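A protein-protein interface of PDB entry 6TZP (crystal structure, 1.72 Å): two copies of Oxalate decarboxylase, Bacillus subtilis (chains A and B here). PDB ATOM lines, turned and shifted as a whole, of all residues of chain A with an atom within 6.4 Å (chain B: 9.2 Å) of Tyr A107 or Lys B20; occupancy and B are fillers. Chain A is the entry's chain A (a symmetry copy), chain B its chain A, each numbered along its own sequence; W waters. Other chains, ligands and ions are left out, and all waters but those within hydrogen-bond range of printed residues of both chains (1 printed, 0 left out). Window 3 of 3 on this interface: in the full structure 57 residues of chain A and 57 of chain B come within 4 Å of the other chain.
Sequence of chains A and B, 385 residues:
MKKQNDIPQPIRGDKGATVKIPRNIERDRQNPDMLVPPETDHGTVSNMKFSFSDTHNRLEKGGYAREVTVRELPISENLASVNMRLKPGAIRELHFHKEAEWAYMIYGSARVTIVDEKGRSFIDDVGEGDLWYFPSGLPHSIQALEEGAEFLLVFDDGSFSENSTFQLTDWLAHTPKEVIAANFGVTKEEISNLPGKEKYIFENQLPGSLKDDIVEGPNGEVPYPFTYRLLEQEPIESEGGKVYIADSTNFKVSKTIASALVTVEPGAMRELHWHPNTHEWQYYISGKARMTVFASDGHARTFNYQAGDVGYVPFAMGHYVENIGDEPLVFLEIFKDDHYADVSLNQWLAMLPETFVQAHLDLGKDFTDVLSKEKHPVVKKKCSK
No position is printed for both chains.
Among the printed residues, pairs that only touch across the chains: Tyr A64 with Pro B10 (3.5 Å), Tyr A64 with Ala B17 (3.5 Å), Tyr A64 with Thr B18 (3.9 Å), Tyr A64 with Val B19 (3.4 Å), Arg A85 with Ala B17 (3.9 Å), Arg A85 with Lys B20 (3.5 Å), Ile A106 with Ile B21 (3.5 Å), Tyr A107 with Lys B20 (3.6 Å) and Glu A150 with Val B19 (3.9 Å).
Water W1 lies within hydrogen-bond range of OH of Tyr A107 (2.8 Å) and NZ of Lys B20 (3.0 Å).
Printed residues of chain B that touch a printed residue of chain A: Pro B10, Ala B17, Thr B18, Val B19, Lys B20 and Ile B21. Of the 18 printed residues of chain A, 5 touch a printed residue of chain B. Printed residues of chain A that touch a printed residue of chain B: Tyr A64, Arg A85, Ile A106, Tyr A107 and Glu A150. Hydrophobic or aromatic side chains of chain A that line the printed part of chain B: Tyr A64, Ile A106 and Tyr A107. Among the printed residues, no Asp or Glu carboxylate lies within 4 Å of a Lys or Arg side-chain nitrogen of the other chain.
Of the printed residues of chain B, Ile A106 touches Ile B21 (3.5 Å). Of the printed residues of chain B, Tyr A107 touches Lys B20 (3.6 Å). Gly A108 touches none of the printed residues of chain B. No residue of chain B comes within 4 Å of Ala A149. Of the printed residues of chain A, Thr B18 touches Tyr A64 and Arg A85. Lys B20 touches just these residues of chain A: Arg A85, Tyr A107 and Glu A150. The nearest residue of chain B that does not touch Tyr A107 is Ile B21 (4.2 Å). The nearest residue of chain A that does not touch Lys B20 is Tyr A64 (4.4 Å). The nearest printed residue of chain B that does not touch Glu A150 is Thr B18 (4.6 Å).
O of Thr B18 lies within hydrogen-bond range of NE of Arg A85, at 2.7 Å. The backbone NH (N) of Lys B20 lies within hydrogen-bond range of the side-chain carboxylate (OE1) of Glu A150 (2.8 Å). N of Ile B21 lies within hydrogen-bond range of OE1 of Glu A150, 3.4 Å away.
The backbone NH (N) of Ala B17 lies within hydrogen-bond range of the backbone carbonyl oxygen (O) of Pro B10. The backbone NH of Ile A106 sits at hydrogen-bond distance from the backbone carbonyl oxygen of Glu A150. O of Tyr A64 lies within hydrogen-bond range of N of Arg A85 (2.9 Å). The side-chain amide oxygen (OE1) of Gln B9 sits at hydrogen-bond distance from the backbone NH (N) of Val B19 (2.9 Å). The backbone NH (N) of Glu A150 is in hydrogen-bond range of the backbone carbonyl oxygen (O) of Tyr A107, at 2.9 Å. O of Glu A147 is in hydrogen-bond range of OH of Tyr A107 (2.8 Å).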
ATOM      1  N   TYR A  64      21.418  18.804  17.607  1.00  0.00           N
ATOM      2  CA  TYR A  64      21.396  17.373  17.895  1.00  0.00           C
ATOM      3  C   TYR A  64      19.965  16.905  18.136  1.00  0.00           C
ATOM      4  O   TYR A  64      19.048  17.702  18.345  1.00  0.00           O
ATOM      5  CB  TYR A  64      22.297  17.020  19.095  1.00  0.00           C
ATOM      6  CG  TYR A  64      21.939  17.625  20.459  1.00  0.00           C
ATOM      7  CD1 TYR A  64      20.813  17.206  21.176  1.00  0.00           C
ATOM      8  CD2 TYR A  64      22.771  18.575  21.054  1.00  0.00           C
ATOM      9  CE1 TYR A  64      20.515  17.740  22.430  1.00  0.00           C
ATOM     10  CE2 TYR A  64      22.477  19.112  22.305  1.00  0.00           C
ATOM     11  CZ  TYR A  64      21.351  18.690  22.982  1.00  0.00           C
ATOM     12  OH  TYR A  64      21.063  19.228  24.217  1.00  0.00           O
ATOM     13  N   ARG A  85      17.752  19.874  19.758  1.00  0.00           N
ATOM     14  CA  ARG A  85      18.458  21.117  20.059  1.00  0.00           C
ATOM     15  C   ARG A  85      18.894  21.762  18.752  1.00  0.00           C
ATOM     16  O   ARG A  85      19.432  21.081  17.875  1.00  0.00           O
ATOM     17  CB  ARG A  85      19.674  20.834  20.938  1.00  0.00           C
ATOM     18  CG  ARG A  85      20.693  21.957  20.982  1.00  0.00           C
ATOM     19  CD  ARG A  85      20.323  23.000  22.013  1.00  0.00           C
ATOM     20  NE  ARG A  85      21.537  23.647  22.526  1.00  0.00           N
ATOM     21  CZ  ARG A  85      22.000  24.824  22.115  1.00  0.00           C
ATOM     22  NH1 ARG A  85      21.346  25.519  21.190  1.00  0.00           N
ATOM     23  NH2 ARG A  85      23.126  25.311  22.639  1.00  0.00           N
ATOM     24  N   LEU A  86      18.666  23.072  18.623  1.00  0.00           N
ATOM     25  CA  LEU A  86      19.065  23.823  17.438  1.00  0.00           C
ATOM     26  C   LEU A  86      19.888  25.027  17.874  1.00  0.00           C
ATOM     27  O   LEU A  86      19.507  25.726  18.815  1.00  0.00           O
ATOM     28  CB  LEU A  86      17.850  24.288  16.632  1.00  0.00           C
ATOM     29  CG  LEU A  86      17.022  23.212  15.928  1.00  0.00           C
ATOM     30  CD1 LEU A  86      15.784  23.842  15.268  1.00  0.00           C
ATOM     31  CD2 LEU A  86      17.849  22.465  14.906  1.00  0.00           C
ATOM     32  N   TYR A 104       6.837  21.019  23.240  1.00  0.00           N
ATOM     33  CA  TYR A 104       6.948  21.972  24.340  1.00  0.00           C
ATOM     34  C   TYR A 104       8.314  22.646  24.268  1.00  0.00           C
ATOM     35  O   TYR A 104       9.342  21.964  24.278  1.00  0.00           O
ATOM     36  CB  TYR A 104       6.767  21.270  25.692  1.00  0.00           C
ATOM     37  CG  TYR A 104       6.878  22.218  26.873  1.00  0.00           C
ATOM     38  CD1 TYR A 104       5.778  22.941  27.299  1.00  0.00           C
ATOM     39  CD2 TYR A 104       8.085  22.406  27.538  1.00  0.00           C
ATOM     40  CE1 TYR A 104       5.872  23.826  28.369  1.00  0.00           C
ATOM     41  CE2 TYR A 104       8.186  23.281  28.616  1.00  0.00           C
ATOM     42  CZ  TYR A 104       7.074  23.982  29.024  1.00  0.00           C
ATOM     43  OH  TYR A 104       7.166  24.861  30.084  1.00  0.00           O
ATOM     44  N   MET A 105       8.332  23.978  24.213  1.00  0.00           N
ATOM     45  CA  MET A 105       9.590  24.723  24.112  1.00  0.00           C
ATOM     46  C   MET A 105      10.175  24.930  25.504  1.00  0.00           C
ATOM     47  O   MET A 105       9.660  25.735  26.285  1.00  0.00           O
ATOM     48  CB  MET A 105       9.363  26.062  23.413  1.00  0.00           C
ATOM     49  CG  MET A 105      10.658  26.873  23.167  1.00  0.00           C
ATOM     50  SD  MET A 105      11.830  26.116  21.985  1.00  0.00           S
ATOM     51  CE  MET A 105      10.696  25.803  20.668  1.00  0.00           C
ATOM     52  N   ILE A 106      11.258  24.209  25.814  1.00  0.00           N
ATOM     53  CA  ILE A 106      11.863  24.298  27.140  1.00  0.00           C
ATOM     54  C   ILE A 106      12.813  25.479  27.222  1.00  0.00           C
ATOM     55  O   ILE A 106      12.844  26.197  28.232  1.00  0.00           O
ATOM     56  CB  ILE A 106      12.592  22.989  27.495  1.00  0.00           C
ATOM     57  CG1 ILE A 106      11.649  21.791  27.403  1.00  0.00           C
ATOM     58  CG2 ILE A 106      13.201  23.087  28.899  1.00  0.00           C
ATOM     59  CD1 ILE A 106      12.408  20.455  27.420  1.00  0.00           C
ATOM     60  N   TYR A 107      13.617  25.683  26.179  1.00  0.00           N
ATOM     61  CA  TYR A 107      14.642  26.716  26.180  1.00  0.00           C
ATOM     62  C   TYR A 107      14.611  27.469  24.854  1.00  0.00           C
ATOM     63  O   TYR A 107      14.487  26.859  23.790  1.00  0.00           O
ATOM     64  CB  TYR A 107      16.046  26.120  26.403  1.00  0.00           C
ATOM     65  CG  TYR A 107      17.121  27.115  26.022  1.00  0.00           C
ATOM     66  CD1 TYR A 107      17.562  28.064  26.932  1.00  0.00           C
ATOM     67  CD2 TYR A 107      17.649  27.147  24.729  1.00  0.00           C
ATOM     68  CE1 TYR A 107      18.519  29.011  26.574  1.00  0.00           C
ATOM     69  CE2 TYR A 107      18.605  28.089  24.368  1.00  0.00           C
ATOM     70  CZ  TYR A 107      19.033  29.017  25.292  1.00  0.00           C
ATOM     71  OH  TYR A 107      19.986  29.954  24.928  1.00  0.00           O
ATOM     72  N   GLY A 108      14.735  28.800  24.914  1.00  0.00           N
ATOM     73  CA  GLY A 108      14.959  29.568  23.700  1.00  0.00           C
ATOM     74  C   GLY A 108      13.684  29.857  22.922  1.00  0.00           C
ATOM     75  O   GLY A 108      12.599  30.023  23.490  1.00  0.00           O
ATOM     76  N   SER A 109      13.824  29.928  21.597  1.00  0.00           N
ATOM     77  CA  SER A 109      12.686  30.253  20.739  1.00  0.00           C
ATOM     78  C   SER A 109      12.959  29.763  19.324  1.00  0.00           C
ATOM     79  O   SER A 109      14.105  29.526  18.941  1.00  0.00           O
ATOM     80  CB  SER A 109      12.399  31.759  20.716  1.00  0.00           C
ATOM     81  OG  SER A 109      13.525  32.501  20.270  1.00  0.00           O
ATOM     82  N   GLY A 127       8.074  30.665  21.935  1.00  0.00           N
ATOM     83  CA  GLY A 127       9.034  30.883  22.989  1.00  0.00           C
ATOM     84  C   GLY A 127       8.884  29.878  24.118  1.00  0.00           C
ATOM     85  O   GLY A 127       8.087  28.940  24.055  1.00  0.00           O
ATOM     86  N   GLU A 128       9.673  30.095  25.175  1.00  0.00           N
ATOM     87  CA  GLU A 128       9.656  29.171  26.309  1.00  0.00           C
ATOM     88  C   GLU A 128       8.255  29.078  26.903  1.00  0.00           C
ATOM     89  O   GLU A 128       7.593  30.094  27.143  1.00  0.00           O
ATOM     90  CB  GLU A 128      10.672  29.604  27.374  1.00  0.00           C
ATOM     91  CG  GLU A 128      12.132  29.396  26.936  1.00  0.00           C
ATOM     92  CD  GLU A 128      13.159  30.010  27.894  1.00  0.00           C
ATOM     93  OE1 GLU A 128      12.761  30.457  28.994  1.00  0.00           O
ATOM     94  OE2 GLU A 128      14.364  30.052  27.536  1.00  0.00           O
ATOM     95  N   GLY A 129       7.801  27.849  27.123  1.00  0.00           N
ATOM     96  CA  GLY A 129       6.479  27.576  27.650  1.00  0.00           C
ATOM     97  C   GLY A 129       5.380  27.502  26.612  1.00  0.00           C
ATOM     98  O   GLY A 129       4.220  27.243  26.973  1.00  0.00           O
ATOM     99  N   GLU A 146      17.600  33.780  17.859  1.00  0.00           N
ATOM    100  CA  GLU A 146      18.934  34.231  18.261  1.00  0.00           C
ATOM    101  C   GLU A 146      19.446  33.566  19.534  1.00  0.00           C
ATOM    102  O   GLU A 146      20.652  33.634  19.815  1.00  0.00           O
ATOM    103  CB  GLU A 146      18.941  35.758  18.430  1.00  0.00           C
ATOM    104  CG  GLU A 146      18.148  36.265  19.641  1.00  0.00           C
ATOM    105  CD  GLU A 146      16.643  36.279  19.420  1.00  0.00           C
ATOM    106  OE1 GLU A 146      16.189  36.217  18.251  1.00  0.00           O
ATOM    107  OE2 GLU A 146      15.909  36.351  20.429  1.00  0.00           O
ATOM    108  N   GLU A 147      18.573  32.940  20.320  1.00  0.00           N
ATOM    109  CA  GLU A 147      19.029  32.222  21.501  1.00  0.00           C
ATOM    110  C   GLU A 147      19.292  30.749  21.227  1.00  0.00           C
ATOM    111  O   GLU A 147      19.785  30.049  22.123  1.00  0.00           O
ATOM    112  CB  GLU A 147      18.008  32.355  22.646  1.00  0.00           C
ATOM    113  CG  GLU A 147      17.898  33.785  23.204  1.00  0.00           C
ATOM    114  CD  GLU A 147      19.184  34.268  23.889  1.00  0.00           C
ATOM    115  OE1 GLU A 147      19.991  33.423  24.331  1.00  0.00           O
ATOM    116  OE2 GLU A 147      19.389  35.501  23.986  1.00  0.00           O
ATOM    117  N   GLY A 148      19.020  30.270  20.011  1.00  0.00           N
ATOM    118  CA  GLY A 148      18.931  28.836  19.827  1.00  0.00           C
ATOM    119  C   GLY A 148      17.623  28.335  20.427  1.00  0.00           C
ATOM    120  O   GLY A 148      16.765  29.104  20.848  1.00  0.00           O
ATOM    121  N   ALA A 149      17.485  27.010  20.472  1.00  0.00           N
ATOM    122  CA  ALA A 149      16.239  26.435  20.965  1.00  0.00           C
ATOM    123  C   ALA A 149      16.501  25.012  21.419  1.00  0.00           C
ATOM    124  O   ALA A 149      17.339  24.318  20.849  1.00  0.00           O
ATOM    125  CB  ALA A 149      15.148  26.446  19.887  1.00  0.00           C
ATOM    126  N   GLU A 150      15.794  24.592  22.462  1.00  0.00           N
ATOM    127  CA  GLU A 150      15.799  23.179  22.830  1.00  0.00           C
ATOM    128  C   GLU A 150      14.407  22.807  23.319  1.00  0.00           C
ATOM    129  O   GLU A 150      13.819  23.516  24.142  1.00  0.00           O
ATOM    130  CB  GLU A 150      16.866  22.856  23.896  1.00  0.00           C
ATOM    131  CG  GLU A 150      16.983  21.326  24.111  1.00  0.00           C
ATOM    132  CD  GLU A 150      18.287  20.880  24.759  1.00  0.00           C
ATOM    133  OE1 GLU A 150      19.063  21.734  25.249  1.00  0.00           O
ATOM    134  OE2 GLU A 150      18.541  19.655  24.761  1.00  0.00           O
ATOM    135  N   PHE A 151      13.879  21.702  22.798  1.00  0.00           N
ATOM    136  CA  PHE A 151      12.461  21.426  22.965  1.00  0.00           C
ATOM    137  C   PHE A 151      12.222  19.924  22.991  1.00  0.00           C
ATOM    138  O   PHE A 151      13.074  19.119  22.599  1.00  0.00           O
ATOM    139  CB  PHE A 151      11.633  22.094  21.853  1.00  0.00           C
ATOM    140  CG  PHE A 151      12.249  21.990  20.475  1.00  0.00           C
ATOM    141  CD1 PHE A 151      13.186  22.926  20.042  1.00  0.00           C
ATOM    142  CD2 PHE A 151      11.895  20.961  19.614  1.00  0.00           C
ATOM    143  CE1 PHE A 151      13.749  22.843  18.764  1.00  0.00           C
ATOM    144  CE2 PHE A 151      12.458  20.870  18.338  1.00  0.00           C
ATOM    145  CZ  PHE A 151      13.382  21.810  17.911  1.00  0.00           C
ATOM    146  N   PRO B   8      30.678  17.329  30.453  1.00  0.00           N
ATOM    147  CA  PRO B   8      30.727  16.914  29.046  1.00  0.00           C
ATOM    148  C   PRO B   8      29.600  17.541  28.244  1.00  0.00           C
ATOM    149  O   PRO B   8      28.531  17.861  28.772  1.00  0.00           O
ATOM    150  CB  PRO B   8      30.574  15.393  29.117  1.00  0.00           C
ATOM    151  CG  PRO B   8      29.773  15.165  30.386  1.00  0.00           C
ATOM    152  CD  PRO B   8      30.186  16.262  31.344  1.00  0.00           C
ATOM    153  N   GLN B   9      29.852  17.712  26.945  1.00  0.00           N
ATOM    154  CA  GLN B   9      28.864  18.290  26.047  1.00  0.00           C
ATOM    155  C   GLN B   9      28.769  17.465  24.775  1.00  0.00           C
ATOM    156  O   GLN B   9      29.770  16.895  24.318  1.00  0.00           O
ATOM    157  CB  GLN B   9      29.212  19.740  25.675  1.00  0.00           C
ATOM    158  CG  GLN B   9      29.244  20.703  26.868  1.00  0.00           C
ATOM    159  CD  GLN B   9      27.861  21.017  27.428  1.00  0.00           C
ATOM    160  OE1 GLN B   9      26.842  20.569  26.900  1.00  0.00           O
ATOM    161  NE2 GLN B   9      27.824  21.815  28.497  1.00  0.00           N
ATOM    162  N   PRO B  10      27.583  17.405  24.173  1.00  0.00           N
ATOM    163  CA  PRO B  10      27.398  16.634  22.927  1.00  0.00           C
ATOM    164  C   PRO B  10      27.863  17.437  21.718  1.00  0.00           C
ATOM    165  O   PRO B  10      27.085  17.922  20.901  1.00  0.00           O
ATOM    166  CB  PRO B  10      25.891  16.347  22.934  1.00  0.00           C
ATOM    167  CG  PRO B  10      25.288  17.473  23.695  1.00  0.00           C
ATOM    168  CD  PRO B  10      26.305  17.889  24.731  1.00  0.00           C
ATOM    169  N   ALA B  17      26.074  20.627  19.968  1.00  0.00           N
ATOM    170  CA  ALA B  17      25.869  21.883  20.691  1.00  0.00           C
ATOM    171  C   ALA B  17      25.848  21.590  22.187  1.00  0.00           C
ATOM    172  O   ALA B  17      25.732  20.435  22.604  1.00  0.00           O
ATOM    173  CB  ALA B  17      24.564  22.558  20.261  1.00  0.00           C
ATOM    174  N   THR B  18      25.951  22.650  22.999  1.00  0.00           N
ATOM    175  CA  THR B  18      25.809  22.468  24.444  1.00  0.00           C
ATOM    176  C   THR B  18      24.364  22.119  24.804  1.00  0.00           C
ATOM    177  O   THR B  18      23.418  22.482  24.096  1.00  0.00           O
ATOM    178  CB  THR B  18      26.227  23.728  25.205  1.00  0.00           C
ATOM    179  OG1 THR B  18      25.483  24.844  24.708  1.00  0.00           O
ATOM    180  CG2 THR B  18      27.725  23.995  25.036  1.00  0.00           C
ATOM    181  N   VAL B  19      24.198  21.383  25.907  1.00  0.00           N
ATOM    182  CA  VAL B  19      22.864  21.102  26.436  1.00  0.00           C
ATOM    183  C   VAL B  19      22.361  22.340  27.164  1.00  0.00           C
ATOM    184  O   VAL B  19      23.051  22.880  28.037  1.00  0.00           O
ATOM    185  CB  VAL B  19      22.890  19.889  27.383  1.00  0.00           C
ATOM    186  CG1 VAL B  19      21.474  19.585  27.866  1.00  0.00           C
ATOM    187  CG2 VAL B  19      23.474  18.679  26.693  1.00  0.00           C
ATOM    188  N   LYS B  20      21.149  22.784  26.827  1.00  0.00           N
ATOM    189  CA  LYS B  20      20.595  23.994  27.416  1.00  0.00           C
ATOM    190  C   LYS B  20      19.483  23.735  28.426  1.00  0.00           C
ATOM    191  O   LYS B  20      19.063  24.678  29.106  1.00  0.00           O
ATOM    192  CB  LYS B  20      20.063  24.923  26.314  1.00  0.00           C
ATOM    193  CG  LYS B  20      21.153  25.574  25.470  1.00  0.00           C
ATOM    194  CD  LYS B  20      21.864  26.679  26.257  1.00  0.00           C
ATOM    195  CE  LYS B  20      22.773  27.504  25.333  1.00  0.00           C
ATOM    196  NZ  LYS B  20      23.537  28.529  26.113  1.00  0.00           N
ATOM    197  N   ILE B  21      18.993  22.502  28.541  1.00  0.00           N
ATOM    198  CA  ILE B  21      17.901  22.163  29.457  1.00  0.00           C
ATOM    199  C   ILE B  21      18.457  21.407  30.658  1.00  0.00           C
ATOM    200  O   ILE B  21      19.609  20.937  30.616  1.00  0.00           O
ATOM    201  CB  ILE B  21      16.824  21.333  28.737  1.00  0.00           C
ATOM    202  CG1 ILE B  21      17.403  19.999  28.265  1.00  0.00           C
ATOM    203  CG2 ILE B  21      16.272  22.104  27.538  1.00  0.00           C
ATOM    204  CD1 ILE B  21      16.360  19.099  27.552  1.00  0.00           C
ATOM    205  N   PRO B  22      17.701  21.278  31.751  1.00  0.00           N
ATOM    206  CA  PRO B  22      18.180  20.465  32.877  1.00  0.00           C
ATOM    207  C   PRO B  22      18.471  19.038  32.424  1.00  0.00           C
ATOM    208  O   PRO B  22      17.772  18.480  31.581  1.00  0.00           O
ATOM    209  CB  PRO B  22      17.021  20.531  33.878  1.00  0.00           C
ATOM    210  CG  PRO B  22      16.325  21.826  33.554  1.00  0.00           C
ATOM    211  CD  PRO B  22      16.402  21.911  32.048  1.00  0.00           C
ATOM    212  N   ARG B  23      19.527  18.452  32.991  1.00  0.00           N
ATOM    213  CA  ARG B  23      20.111  17.244  32.424  1.00  0.00           C
ATOM    214  C   ARG B  23      20.665  16.357  33.532  1.00  0.00           C
ATOM    215  O   ARG B  23      20.793  16.770  34.689  1.00  0.00           O
ATOM    216  CB  ARG B  23      21.225  17.589  31.429  1.00  0.00           C
ATOM    217  CG  ARG B  23      22.367  18.354  32.078  1.00  0.00           C
ATOM    218  CD  ARG B  23      23.378  18.888  31.070  1.00  0.00           C
ATOM    219  NE  ARG B  23      24.131  17.812  30.447  1.00  0.00           N
ATOM    220  CZ  ARG B  23      25.325  17.966  29.883  1.00  0.00           C
ATOM    221  NH1 ARG B  23      25.909  19.167  29.854  1.00  0.00           N
ATOM    222  NH2 ARG B  23      25.931  16.918  29.349  1.00  0.00           N
HETATM  223  O   HOH W   1      21.939  30.964  26.696  1.00  0.00           O
